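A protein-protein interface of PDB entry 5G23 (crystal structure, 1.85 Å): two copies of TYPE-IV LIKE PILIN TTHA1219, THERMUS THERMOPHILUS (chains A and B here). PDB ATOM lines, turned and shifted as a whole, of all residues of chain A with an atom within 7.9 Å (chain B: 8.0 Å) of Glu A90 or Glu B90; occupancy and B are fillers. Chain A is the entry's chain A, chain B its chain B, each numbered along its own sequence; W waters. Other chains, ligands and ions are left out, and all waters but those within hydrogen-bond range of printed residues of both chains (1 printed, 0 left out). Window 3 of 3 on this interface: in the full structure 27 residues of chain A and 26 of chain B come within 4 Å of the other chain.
The side-chain sulfur of Met B93 lies within hydrogen-bond range of the side-chain hydroxyl of Tyr A65.
The side-chain carboxylate of Glu A90 lies close to the side-chain carboxylate of Glu B90.
The side-chain carboxylate (OE1) of Glu A90 is in hydrogen-bond range of the side-chain hydroxyl (OH) of Tyr A65.
The side-chain carboxylate of Glu A90 is in salt-bridge range of the guanidinium group of Arg A66, 3.0 Å away.
N of Leu B88 sits at hydrogen-bond distance from O of Tyr B65 (2.9 Å).
The side-chain carboxylate (OE1) of Glu B90 lies within hydrogen-bond range of the side-chain hydroxyl (OH) of Tyr B65 (2.7 Å).
SG of Cys A97 is disulfide-bonded to SG of Cys A89 (2.0 Å).
The side-chain sulfur of Cys B97 is disulfide-bonded to the side-chain sulfur of Cys B89 (2.1 Å).
Of the printed residues of chain B, Glu A90 touches Glu B90 (2.8 Å).
Of chain A, only Tyr A65 (3.8 Å) and Glu A90 (2.8 Å) come within 4 Å of Glu B90.
Printed residues of chain A within 4 Å of Ala B91: Tyr A65 (3.7 Å).
Of the printed residues of chain B, Glu A95 touches Tyr B61 (3.5 Å).
Printed residues of chain A within 4 Å of Glu B95: Tyr A61.
Leu A88 touches none of the printed residues of chain B.
The nearest printed residue of chain A that does not touch Glu B95 is Met A93 (9.1 Å).
Water W1 lies within hydrogen-bond range of the guanidinium group of Arg A66 (3.0 Å), the side-chain carboxylate of Glu A90 (3.0 Å) and the side-chain carboxylate of Glu B90 (3.4 Å).
Tyr A61 touches Glu B94, and with the chains exchanged Glu A94 touches Tyr B61.
Tyr A65 touches Glu B90, but with the chains exchanged Glu A90 does not touch Tyr B65 (4.03 Å).
Tyr A65 touches Met B93, but with the chains exchanged Met A93 does not touch Tyr B65 (5.1 Å).
Met A93 touches Tyr B61, but with the chains exchanged Tyr A61 does not touch Met B93 (4.2 Å).
16 positions are printed for both chains.
Of the 16 pairs that touch across the chains among the printed residues, 10 have their exchanged pair printed and touching as well.
Glu B95 touches Tyr A61.
Tyr A61 touches Gly B98.
OH of Tyr A65 touches OE2 of Glu B90, at 3.8 Å.
Tyr A65 touches Ala B91.
Gly B92 touches Tyr A65.
CE2 of Tyr B61 touches O of Gly A92, at 3.6 Å.
Gly A92 touches Tyr B65 (O to CD1, 3.9 Å).
C of Met A93 touches CE2 of Tyr B61, at 3.9 Å.
CE of Met B93 touches CB of Met A93, 3.4 Å away.
Glu A94 touches Tyr B61 (C to CE2, 3.5 Å).
Of the 18 printed residues of chain B, 9 touch a printed residue of chain A.
Printed residues of chain B that touch a printed residue of chain A: Tyr B61, Tyr B65, Glu B90, Ala B91, Gly B92, Met B93, Glu B94, Glu B95 and Gly B98.
Along chain B the printed residues that touch a printed residue of chain A span positions 61 to 98.
Among the printed residues, 16 pairs touch across the chains.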
ATOM      1  N   TYR A  61       3.808  15.525   5.002  1.00  0.00           N
ATOM      2  CA  TYR A  61       2.637  16.294   5.357  1.00  0.00           C
ATOM      3  C   TYR A  61       2.194  16.035   6.792  1.00  0.00           C
ATOM      4  O   TYR A  61       1.699  16.928   7.431  1.00  0.00           O
ATOM      5  CB  TYR A  61       1.438  15.903   4.426  1.00  0.00           C
ATOM      6  CG  TYR A  61       0.221  16.697   4.655  1.00  0.00           C
ATOM      7  CD1 TYR A  61       0.039  17.933   4.017  1.00  0.00           C
ATOM      8  CD2 TYR A  61      -0.774  16.241   5.498  1.00  0.00           C
ATOM      9  CE1 TYR A  61      -1.116  18.692   4.202  1.00  0.00           C
ATOM     10  CE2 TYR A  61      -1.948  16.987   5.694  1.00  0.00           C
ATOM     11  CZ  TYR A  61      -2.084  18.212   5.057  1.00  0.00           C
ATOM     12  OH  TYR A  61      -3.269  18.946   5.244  1.00  0.00           O
ATOM     13  N   TYR A  65       2.206  16.409  13.445  1.00  0.00           N
ATOM     14  CA  TYR A  65       0.817  16.102  13.811  1.00  0.00           C
ATOM     15  C   TYR A  65       0.720  15.791  15.289  1.00  0.00           C
ATOM     16  O   TYR A  65       1.315  14.842  15.764  1.00  0.00           O
ATOM     17  CB  TYR A  65       0.282  14.922  12.983  1.00  0.00           C
ATOM     18  CG  TYR A  65      -1.193  14.632  13.257  1.00  0.00           C
ATOM     19  CD1 TYR A  65      -2.176  15.534  12.859  1.00  0.00           C
ATOM     20  CD2 TYR A  65      -1.579  13.521  13.952  1.00  0.00           C
ATOM     21  CE1 TYR A  65      -3.509  15.310  13.105  1.00  0.00           C
ATOM     22  CE2 TYR A  65      -2.913  13.285  14.199  1.00  0.00           C
ATOM     23  CZ  TYR A  65      -3.872  14.194  13.777  1.00  0.00           C
ATOM     24  OH  TYR A  65      -5.225  13.960  14.057  1.00  0.00           O
ATOM     25  N   ARG A  66      -0.087  16.620  15.963  1.00  0.00           N
ATOM     26  CA  ARG A  66      -0.373  16.572  17.391  1.00  0.00           C
ATOM     27  C   ARG A  66       0.888  16.441  18.237  1.00  0.00           C
ATOM     28  O   ARG A  66       0.858  15.764  19.270  1.00  0.00           O
ATOM     29  CB  ARG A  66      -1.408  15.488  17.719  1.00  0.00           C
ATOM     30  CG  ARG A  66      -2.704  15.762  16.991  1.00  0.00           C
ATOM     31  CD  ARG A  66      -3.745  14.704  17.220  1.00  0.00           C
ATOM     32  NE  ARG A  66      -3.912  14.414  18.640  1.00  0.00           N
ATOM     33  CZ  ARG A  66      -4.553  13.358  19.131  1.00  0.00           C
ATOM     34  NH1 ARG A  66      -5.131  12.460  18.331  1.00  0.00           N
ATOM     35  NH2 ARG A  66      -4.602  13.190  20.432  1.00  0.00           N
ATOM     36  N   PHE A  87       6.019  12.838  14.415  1.00  0.00           N
ATOM     37  CA  PHE A  87       4.580  13.056  14.544  1.00  0.00           C
ATOM     38  C   PHE A  87       3.975  12.047  15.492  1.00  0.00           C
ATOM     39  O   PHE A  87       4.568  10.991  15.750  1.00  0.00           O
ATOM     40  CB  PHE A  87       3.851  12.942  13.177  1.00  0.00           C
ATOM     41  CG  PHE A  87       4.097  11.642  12.476  1.00  0.00           C
ATOM     42  CD1 PHE A  87       5.243  11.451  11.779  1.00  0.00           C
ATOM     43  CD2 PHE A  87       3.162  10.584  12.553  1.00  0.00           C
ATOM     44  CE1 PHE A  87       5.482  10.240  11.131  1.00  0.00           C
ATOM     45  CE2 PHE A  87       3.393   9.356  11.921  1.00  0.00           C
ATOM     46  CZ  PHE A  87       4.572   9.184  11.198  1.00  0.00           C
ATOM     47  N   LEU A  88       2.782  12.365  15.988  1.00  0.00           N
ATOM     48  CA  LEU A  88       2.049  11.440  16.830  1.00  0.00           C
ATOM     49  C   LEU A  88       1.214  10.511  15.950  1.00  0.00           C
ATOM     50  O   LEU A  88       0.506  10.971  15.080  1.00  0.00           O
ATOM     51  CB  LEU A  88       1.157  12.220  17.780  1.00  0.00           C
ATOM     52  CG  LEU A  88       0.431  11.342  18.822  1.00  0.00           C
ATOM     53  CD1 LEU A  88       1.445  10.840  19.833  1.00  0.00           C
ATOM     54  CD2 LEU A  88      -0.664  12.118  19.534  1.00  0.00           C
ATOM     55  N   CYS A  89       1.275   9.210  16.196  1.00  0.00           N
ATOM     56  CA  CYS A  89       0.328   8.209  15.572  1.00  0.00           C
ATOM     57  C   CYS A  89      -1.092   8.115  16.230  1.00  0.00           C
ATOM     58  O   CYS A  89      -1.190   7.912  17.434  1.00  0.00           O
ATOM     59  CB  CYS A  89       0.927   6.839  15.658  1.00  0.00           C
ATOM     60  SG  CYS A  89       1.867   6.403  14.159  1.00  0.00           S
ATOM     61  N   GLU A  90      -2.162   8.337  15.460  1.00  0.00           N
ATOM     62  CA  GLU A  90      -3.600   8.232  15.917  1.00  0.00           C
ATOM     63  C   GLU A  90      -4.082   6.966  15.257  1.00  0.00           C
ATOM     64  O   GLU A  90      -3.879   6.801  14.072  1.00  0.00           O
ATOM     65  CB  GLU A  90      -4.497   9.444  15.434  1.00  0.00           C
ATOM     66  CG  GLU A  90      -6.060   9.495  15.722  1.00  0.00           C
ATOM     67  CD  GLU A  90      -6.652  10.942  15.618  1.00  0.00           C
ATOM     68  OE1 GLU A  90      -5.775  11.792  15.463  1.00  0.00           O
ATOM     69  OE2 GLU A  90      -7.909  11.303  15.714  1.00  0.00           O
ATOM     70  N   ALA A  91      -4.718   6.076  16.020  1.00  0.00           N
ATOM     71  CA  ALA A  91      -5.276   4.853  15.463  1.00  0.00           C
ATOM     72  C   ALA A  91      -6.081   5.136  14.186  1.00  0.00           C
ATOM     73  O   ALA A  91      -6.793   6.152  14.098  1.00  0.00           O
ATOM     74  CB  ALA A  91      -6.155   4.177  16.496  1.00  0.00           C
ATOM     75  N   GLY A  92      -5.988   4.245  13.197  1.00  0.00           N
ATOM     76  CA  GLY A  92      -6.825   4.351  11.993  1.00  0.00           C
ATOM     77  C   GLY A  92      -6.355   5.379  10.978  1.00  0.00           C
ATOM     78  O   GLY A  92      -6.982   5.539   9.933  1.00  0.00           O
ATOM     79  N   MET A  93      -5.236   6.049  11.256  1.00  0.00           N
ATOM     80  CA  MET A  93      -4.573   6.985  10.309  1.00  0.00           C
ATOM     81  C   MET A  93      -3.648   6.240   9.361  1.00  0.00           C
ATOM     82  O   MET A  93      -3.651   6.501   8.158  1.00  0.00           O
ATOM     83  CB  MET A  93      -3.728   8.036  11.085  1.00  0.00           C
ATOM     84  CG  MET A  93      -2.776   8.951  10.247  1.00  0.00           C
ATOM     85  SD  MET A  93      -1.792  10.276  11.124  1.00  0.00           S
ATOM     86  CE  MET A  93      -1.461   9.523  12.717  1.00  0.00           C
ATOM     87  N   GLU A  94      -2.808   5.374   9.921  1.00  0.00           N
ATOM     88  CA  GLU A  94      -1.903   4.568   9.148  1.00  0.00           C
ATOM     89  C   GLU A  94      -1.758   3.192   9.762  1.00  0.00           C
ATOM     90  O   GLU A  94      -1.784   3.019  10.976  1.00  0.00           O
ATOM     91  CB  GLU A  94      -0.493   5.188   9.069  1.00  0.00           C
ATOM     92  CG  GLU A  94      -0.303   6.546   8.475  1.00  0.00           C
ATOM     93  CD  GLU A  94       1.102   7.049   8.737  1.00  0.00           C
ATOM     94  OE1 GLU A  94       2.050   6.356   8.332  1.00  0.00           O
ATOM     95  OE2 GLU A  94       1.258   8.137   9.328  1.00  0.00           O
ATOM     96  N   GLU A  95      -1.526   2.227   8.884  1.00  0.00           N
ATOM     97  CA  GLU A  95      -1.249   0.847   9.257  1.00  0.00           C
ATOM     98  C   GLU A  95      -0.099   0.747  10.288  1.00  0.00           C
ATOM     99  O   GLU A  95      -0.220   0.027  11.276  1.00  0.00           O
ATOM    100  CB  GLU A  95      -0.915   0.033   7.982  1.00  0.00           C
ATOM    101  CG  GLU A  95      -1.472  -1.393   7.918  1.00  0.00           C
ATOM    102  CD  GLU A  95      -0.638  -2.419   8.650  1.00  0.00           C
ATOM    103  OE1 GLU A  95       0.480  -2.069   9.146  1.00  0.00           O
ATOM    104  OE2 GLU A  95      -1.089  -3.593   8.673  1.00  0.00           O
ATOM    105  N   CYS A  97       0.956   2.604  12.487  1.00  0.00           N
ATOM    106  CA  CYS A  97       0.580   3.096  13.815  1.00  0.00           C
ATOM    107  C   CYS A  97      -0.133   2.022  14.602  1.00  0.00           C
ATOM    108  O   CYS A  97      -0.327   2.204  15.779  1.00  0.00           O
ATOM    109  CB  CYS A  97      -0.331   4.331  13.713  1.00  0.00           C
ATOM    110  SG  CYS A  97       0.398   5.798  12.950  1.00  0.00           S
ATOM    111  N   MET A 101      -0.581   3.333  18.641  1.00  0.00           N
ATOM    112  CA  MET A 101      -1.600   4.317  19.007  1.00  0.00           C
ATOM    113  C   MET A 101      -1.151   5.237  20.154  1.00  0.00           C
ATOM    114  O   MET A 101      -0.744   4.776  21.216  1.00  0.00           O
ATOM    115  CB  MET A 101      -2.908   3.591  19.343  1.00  0.00           C
ATOM    116  CG  MET A 101      -3.492   2.815  18.161  1.00  0.00           C
ATOM    117  SD  MET A 101      -3.237   1.025  18.161  1.00  0.00           S
ATOM    118  CE  MET A 101      -4.499   0.444  17.022  1.00  0.00           C
ATOM    119  N   GLY A 102      -1.178   6.547  19.912  1.00  0.00           N
ATOM    120  CA  GLY A 102      -0.748   7.535  20.892  1.00  0.00           C
ATOM    121  C   GLY A 102       0.759   7.585  21.129  1.00  0.00           C
ATOM    122  O   GLY A 102       1.208   8.103  22.159  1.00  0.00           O
ATOM    123  N   GLU A 103       1.533   7.076  20.164  1.00  0.00           N
ATOM    124  CA  GLU A 103       3.005   7.042  20.214  1.00  0.00           C
ATOM    125  C   GLU A 103       3.673   7.931  19.109  1.00  0.00           C
ATOM    126  O   GLU A 103       3.208   7.994  17.975  1.00  0.00           O
ATOM    127  CB  GLU A 103       3.484   5.572  20.155  1.00  0.00           C
ATOM    128  CG  GLU A 103       3.937   5.037  18.756  1.00  0.00           C
ATOM    129  CD  GLU A 103       3.158   3.862  18.088  1.00  0.00           C
ATOM    130  OE1 GLU A 103       2.125   3.367  18.587  1.00  0.00           O
ATOM    131  OE2 GLU A 103       3.619   3.401  17.013  1.00  0.00           O
ATOM    132  N   TYR B  61      -6.025   2.257   2.903  1.00  0.00           N
ATOM    133  CA  TYR B  61      -6.170   1.982   4.325  1.00  0.00           C
ATOM    134  C   TYR B  61      -7.208   2.928   4.957  1.00  0.00           C
ATOM    135  O   TYR B  61      -7.893   2.561   5.885  1.00  0.00           O
ATOM    136  CB  TYR B  61      -4.838   2.180   5.032  1.00  0.00           C
ATOM    137  CG  TYR B  61      -4.880   1.917   6.499  1.00  0.00           C
ATOM    138  CD1 TYR B  61      -4.756   0.621   6.977  1.00  0.00           C
ATOM    139  CD2 TYR B  61      -5.039   2.945   7.421  1.00  0.00           C
ATOM    140  CE1 TYR B  61      -4.775   0.347   8.336  1.00  0.00           C
ATOM    141  CE2 TYR B  61      -5.035   2.691   8.778  1.00  0.00           C
ATOM    142  CZ  TYR B  61      -4.927   1.359   9.228  1.00  0.00           C
ATOM    143  OH  TYR B  61      -4.965   1.058  10.570  1.00  0.00           O
ATOM    144  N   TYR B  65     -13.095   5.821   6.628  1.00  0.00           N
ATOM    145  CA  TYR B  65     -12.753   6.529   7.870  1.00  0.00           C
ATOM    146  C   TYR B  65     -13.809   7.536   8.226  1.00  0.00           C
ATOM    147  O   TYR B  65     -14.091   8.448   7.443  1.00  0.00           O
ATOM    148  CB  TYR B  65     -11.425   7.234   7.712  1.00  0.00           C
ATOM    149  CG  TYR B  65     -10.944   7.910   8.971  1.00  0.00           C
ATOM    150  CD1 TYR B  65     -10.501   7.144  10.050  1.00  0.00           C
ATOM    151  CD2 TYR B  65     -10.930   9.276   9.079  1.00  0.00           C
ATOM    152  CE1 TYR B  65     -10.043   7.742  11.214  1.00  0.00           C
ATOM    153  CE2 TYR B  65     -10.497   9.891  10.243  1.00  0.00           C
ATOM    154  CZ  TYR B  65     -10.050   9.115  11.297  1.00  0.00           C
ATOM    155  OH  TYR B  65      -9.647   9.726  12.441  1.00  0.00           O
ATOM    156  N   ARG B  66     -14.419   7.310   9.382  1.00  0.00           N
ATOM    157  CA  ARG B  66     -15.492   8.101   9.971  1.00  0.00           C
ATOM    158  C   ARG B  66     -16.624   8.363   8.995  1.00  0.00           C
ATOM    159  O   ARG B  66     -17.242   9.404   9.060  1.00  0.00           O
ATOM    160  CB  ARG B  66     -14.919   9.381  10.610  1.00  0.00           C
ATOM    161  CG  ARG B  66     -13.893   9.077  11.703  1.00  0.00           C
ATOM    162  CD  ARG B  66     -13.242  10.308  12.317  1.00  0.00           C
ATOM    163  NE  ARG B  66     -14.231  11.299  12.712  1.00  0.00           N
ATOM    164  CZ  ARG B  66     -13.964  12.582  12.983  1.00  0.00           C
ATOM    165  NH1 ARG B  66     -12.710  13.053  12.969  1.00  0.00           N
ATOM    166  NH2 ARG B  66     -14.955  13.396  13.292  1.00  0.00           N
ATOM    167  N   PHE B  87     -13.881   8.493   2.112  1.00  0.00           N
ATOM    168  CA  PHE B  87     -13.565   8.662   3.538  1.00  0.00           C
ATOM    169  C   PHE B  87     -13.789  10.114   3.945  1.00  0.00           C
ATOM    170  O   PHE B  87     -13.851  11.011   3.103  1.00  0.00           O
ATOM    171  CB  PHE B  87     -12.125   8.262   3.837  1.00  0.00           C
ATOM    172  CG  PHE B  87     -11.117   8.981   2.953  1.00  0.00           C
ATOM    173  CD1 PHE B  87     -10.845   8.542   1.679  1.00  0.00           C
ATOM    174  CD2 PHE B  87     -10.468  10.089   3.409  1.00  0.00           C
ATOM    175  CE1 PHE B  87      -9.935   9.219   0.836  1.00  0.00           C
ATOM    176  CE2 PHE B  87      -9.524  10.757   2.610  1.00  0.00           C
ATOM    177  CZ  PHE B  87      -9.288  10.334   1.315  1.00  0.00           C
ATOM    178  N   LEU B  88     -13.914  10.332   5.246  1.00  0.00           N
ATOM    179  CA  LEU B  88     -14.050  11.643   5.816  1.00  0.00           C
ATOM    180  C   LEU B  88     -12.682  12.219   6.092  1.00  0.00           C
ATOM    181  O   LEU B  88     -11.813  11.568   6.626  1.00  0.00           O
ATOM    182  CB  LEU B  88     -14.794  11.588   7.136  1.00  0.00           C
ATOM    183  CG  LEU B  88     -15.123  12.978   7.717  1.00  0.00           C
ATOM    184  CD1 LEU B  88     -16.190  13.661   6.901  1.00  0.00           C
ATOM    185  CD2 LEU B  88     -15.558  12.898   9.174  1.00  0.00           C
ATOM    186  N   CYS B  89     -12.471  13.441   5.693  1.00  0.00           N
ATOM    187  CA  CYS B  89     -11.221  14.114   5.992  1.00  0.00           C
ATOM    188  C   CYS B  89     -11.165  14.728   7.390  1.00  0.00           C
ATOM    189  O   CYS B  89     -12.027  15.490   7.717  1.00  0.00           O
ATOM    190  CB  CYS B  89     -11.012  15.182   4.941  1.00  0.00           C
ATOM    191  SG  CYS B  89     -10.446  14.494   3.433  1.00  0.00           S
ATOM    192  N   GLU B  90     -10.111  14.426   8.156  1.00  0.00           N
ATOM    193  CA  GLU B  90      -9.745  15.099   9.438  1.00  0.00           C
ATOM    194  C   GLU B  90      -8.482  15.931   9.150  1.00  0.00           C
ATOM    195  O   GLU B  90      -7.502  15.413   8.588  1.00  0.00           O
ATOM    196  CB  GLU B  90      -9.404  14.070  10.549  1.00  0.00           C
ATOM    197  CG  GLU B  90      -9.017  14.567  11.995  1.00  0.00           C
ATOM    198  CD  GLU B  90      -9.241  13.452  13.082  1.00  0.00           C
ATOM    199  OE1 GLU B  90      -9.775  12.387  12.619  1.00  0.00           O
ATOM    200  OE2 GLU B  90      -8.942  13.557  14.348  1.00  0.00           O
ATOM    201  N   ALA B  91      -8.502  17.205   9.500  1.00  0.00           N
ATOM    202  CA  ALA B  91      -7.336  18.071   9.283  1.00  0.00           C
ATOM    203  C   ALA B  91      -6.012  17.458   9.801  1.00  0.00           C
ATOM    204  O   ALA B  91      -5.994  16.794  10.839  1.00  0.00           O
ATOM    205  CB  ALA B  91      -7.562  19.417   9.939  1.00  0.00           C
ATOM    206  N   GLY B  92      -4.929  17.668   9.052  1.00  0.00           N
ATOM    207  CA  GLY B  92      -3.588  17.359   9.509  1.00  0.00           C
ATOM    208  C   GLY B  92      -3.109  15.951   9.183  1.00  0.00           C
ATOM    209  O   GLY B  92      -1.900  15.683   9.257  1.00  0.00           O
ATOM    210  N   MET B  93      -4.029  15.070   8.823  1.00  0.00           N
ATOM    211  CA  MET B  93      -3.715  13.623   8.652  1.00  0.00           C
ATOM    212  C   MET B  93      -3.252  13.265   7.240  1.00  0.00           C
ATOM    213  O   MET B  93      -2.257  12.557   7.069  1.00  0.00           O
ATOM    214  CB  MET B  93      -4.906  12.736   9.125  1.00  0.00           C
ATOM    215  CG  MET B  93      -4.881  12.466  10.647  1.00  0.00           C
ATOM    216  SD  MET B  93      -6.194  11.467  11.452  1.00  0.00           S
ATOM    217  CE  MET B  93      -6.412  10.027  10.399  1.00  0.00           C
ATOM    218  N   GLU B  94      -3.954  13.760   6.223  1.00  0.00           N
ATOM    219  CA  GLU B  94      -3.759  13.320   4.861  1.00  0.00           C
ATOM    220  C   GLU B  94      -3.668  14.539   3.957  1.00  0.00           C
ATOM    221  O   GLU B  94      -4.469  15.466   4.049  1.00  0.00           O
ATOM    222  CB  GLU B  94      -4.847  12.353   4.397  1.00  0.00           C
ATOM    223  CG  GLU B  94      -5.048  11.149   5.410  1.00  0.00           C
ATOM    224  CD  GLU B  94      -4.055   9.965   5.224  1.00  0.00           C
ATOM    225  OE1 GLU B  94      -4.034   9.386   4.100  1.00  0.00           O
ATOM    226  OE2 GLU B  94      -3.283   9.588   6.176  1.00  0.00           O
ATOM    227  N   GLU B  95      -2.627  14.557   3.121  1.00  0.00           N
ATOM    228  CA  GLU B  95      -2.332  15.681   2.289  1.00  0.00           C
ATOM    229  C   GLU B  95      -3.521  16.113   1.440  1.00  0.00           C
ATOM    230  O   GLU B  95      -3.805  17.289   1.339  1.00  0.00           O
ATOM    231  CB  GLU B  95      -1.171  15.328   1.341  1.00  0.00           C
ATOM    232  CG  GLU B  95      -0.484  16.532   0.755  1.00  0.00           C
ATOM    233  CD  GLU B  95       0.509  16.216  -0.341  1.00  0.00           C
ATOM    234  OE1 GLU B  95       0.668  14.987  -0.672  1.00  0.00           O
ATOM    235  OE2 GLU B  95       1.164  17.185  -0.808  1.00  0.00           O
ATOM    236  N   CYS B  97      -6.597  15.816   1.886  1.00  0.00           N
ATOM    237  CA  CYS B  97      -7.607  16.438   2.742  1.00  0.00           C
ATOM    238  C   CYS B  97      -7.331  17.885   3.072  1.00  0.00           C
ATOM    239  O   CYS B  97      -8.178  18.536   3.598  1.00  0.00           O
ATOM    240  CB  CYS B  97      -7.755  15.683   4.082  1.00  0.00           C
ATOM    241  SG  CYS B  97      -8.483  14.052   3.841  1.00  0.00           S
ATOM    242  N   GLY B  98      -6.132  18.376   2.812  1.00  0.00           N
ATOM    243  CA  GLY B  98      -5.804  19.781   3.014  1.00  0.00           C
ATOM    244  C   GLY B  98      -6.877  20.868   3.021  1.00  0.00           C
ATOM    245  O   GLY B  98      -6.843  21.740   3.889  1.00  0.00           O
ATOM    246  N   SER B 100     -10.385  19.967   2.839  1.00  0.00           N
ATOM    247  CA  SER B 100     -11.634  19.225   2.911  1.00  0.00           C
ATOM    248  C   SER B 100     -11.901  18.774   4.316  1.00  0.00           C
ATOM    249  O   SER B 100     -12.572  17.750   4.507  1.00  0.00           O
ATOM    250  CB  SER B 100     -11.625  18.018   1.970  1.00  0.00           C
ATOM    251  OG  SER B 100     -11.142  18.346   0.691  1.00  0.00           O
ATOM    252  N   MET B 101     -11.414  19.539   5.296  1.00  0.00           N
ATOM    253  CA  MET B 101     -11.658  19.235   6.711  1.00  0.00           C
ATOM    254  C   MET B 101     -13.164  18.977   7.035  1.00  0.00           C
ATOM    255  O   MET B 101     -14.036  19.798   6.727  1.00  0.00           O
ATOM    256  CB  MET B 101     -11.086  20.374   7.559  1.00  0.00           C
ATOM    257  CG  MET B 101      -9.570  20.537   7.399  1.00  0.00           C
ATOM    258  SD  MET B 101      -9.021  21.881   6.300  1.00  0.00           S
ATOM    259  CE  MET B 101      -7.329  22.161   6.862  1.00  0.00           C
ATOM    260  N   GLY B 102     -13.471  17.816   7.625  1.00  0.00           N
ATOM    261  CA  GLY B 102     -14.860  17.426   7.911  1.00  0.00           C
ATOM    262  C   GLY B 102     -15.725  17.151   6.698  1.00  0.00           C
ATOM    263  O   GLY B 102     -16.956  17.132   6.771  1.00  0.00           O
ATOM    264  N   GLU B 103     -15.075  16.961   5.572  1.00  0.00           N
ATOM    265  CA  GLU B 103     -15.747  16.672   4.289  1.00  0.00           C
ATOM    266  C   GLU B 103     -15.318  15.322   3.694  1.00  0.00           C
ATOM    267  O   GLU B 103     -14.179  14.880   3.858  1.00  0.00           O
ATOM    268  CB  GLU B 103     -15.479  17.849   3.344  1.00  0.00           C
ATOM    269  CG  GLU B 103     -16.280  19.059   3.786  1.00  0.00           C
ATOM    270  CD  GLU B 103     -15.887  20.363   3.078  1.00  0.00           C
ATOM    271  OE1 GLU B 103     -14.894  20.377   2.275  1.00  0.00           O
ATOM    272  OE2 GLU B 103     -16.586  21.379   3.364  1.00  0.00           O
HETATM  273  O   HOH W   1      -7.746  13.716  17.516  1.00  0.00           O
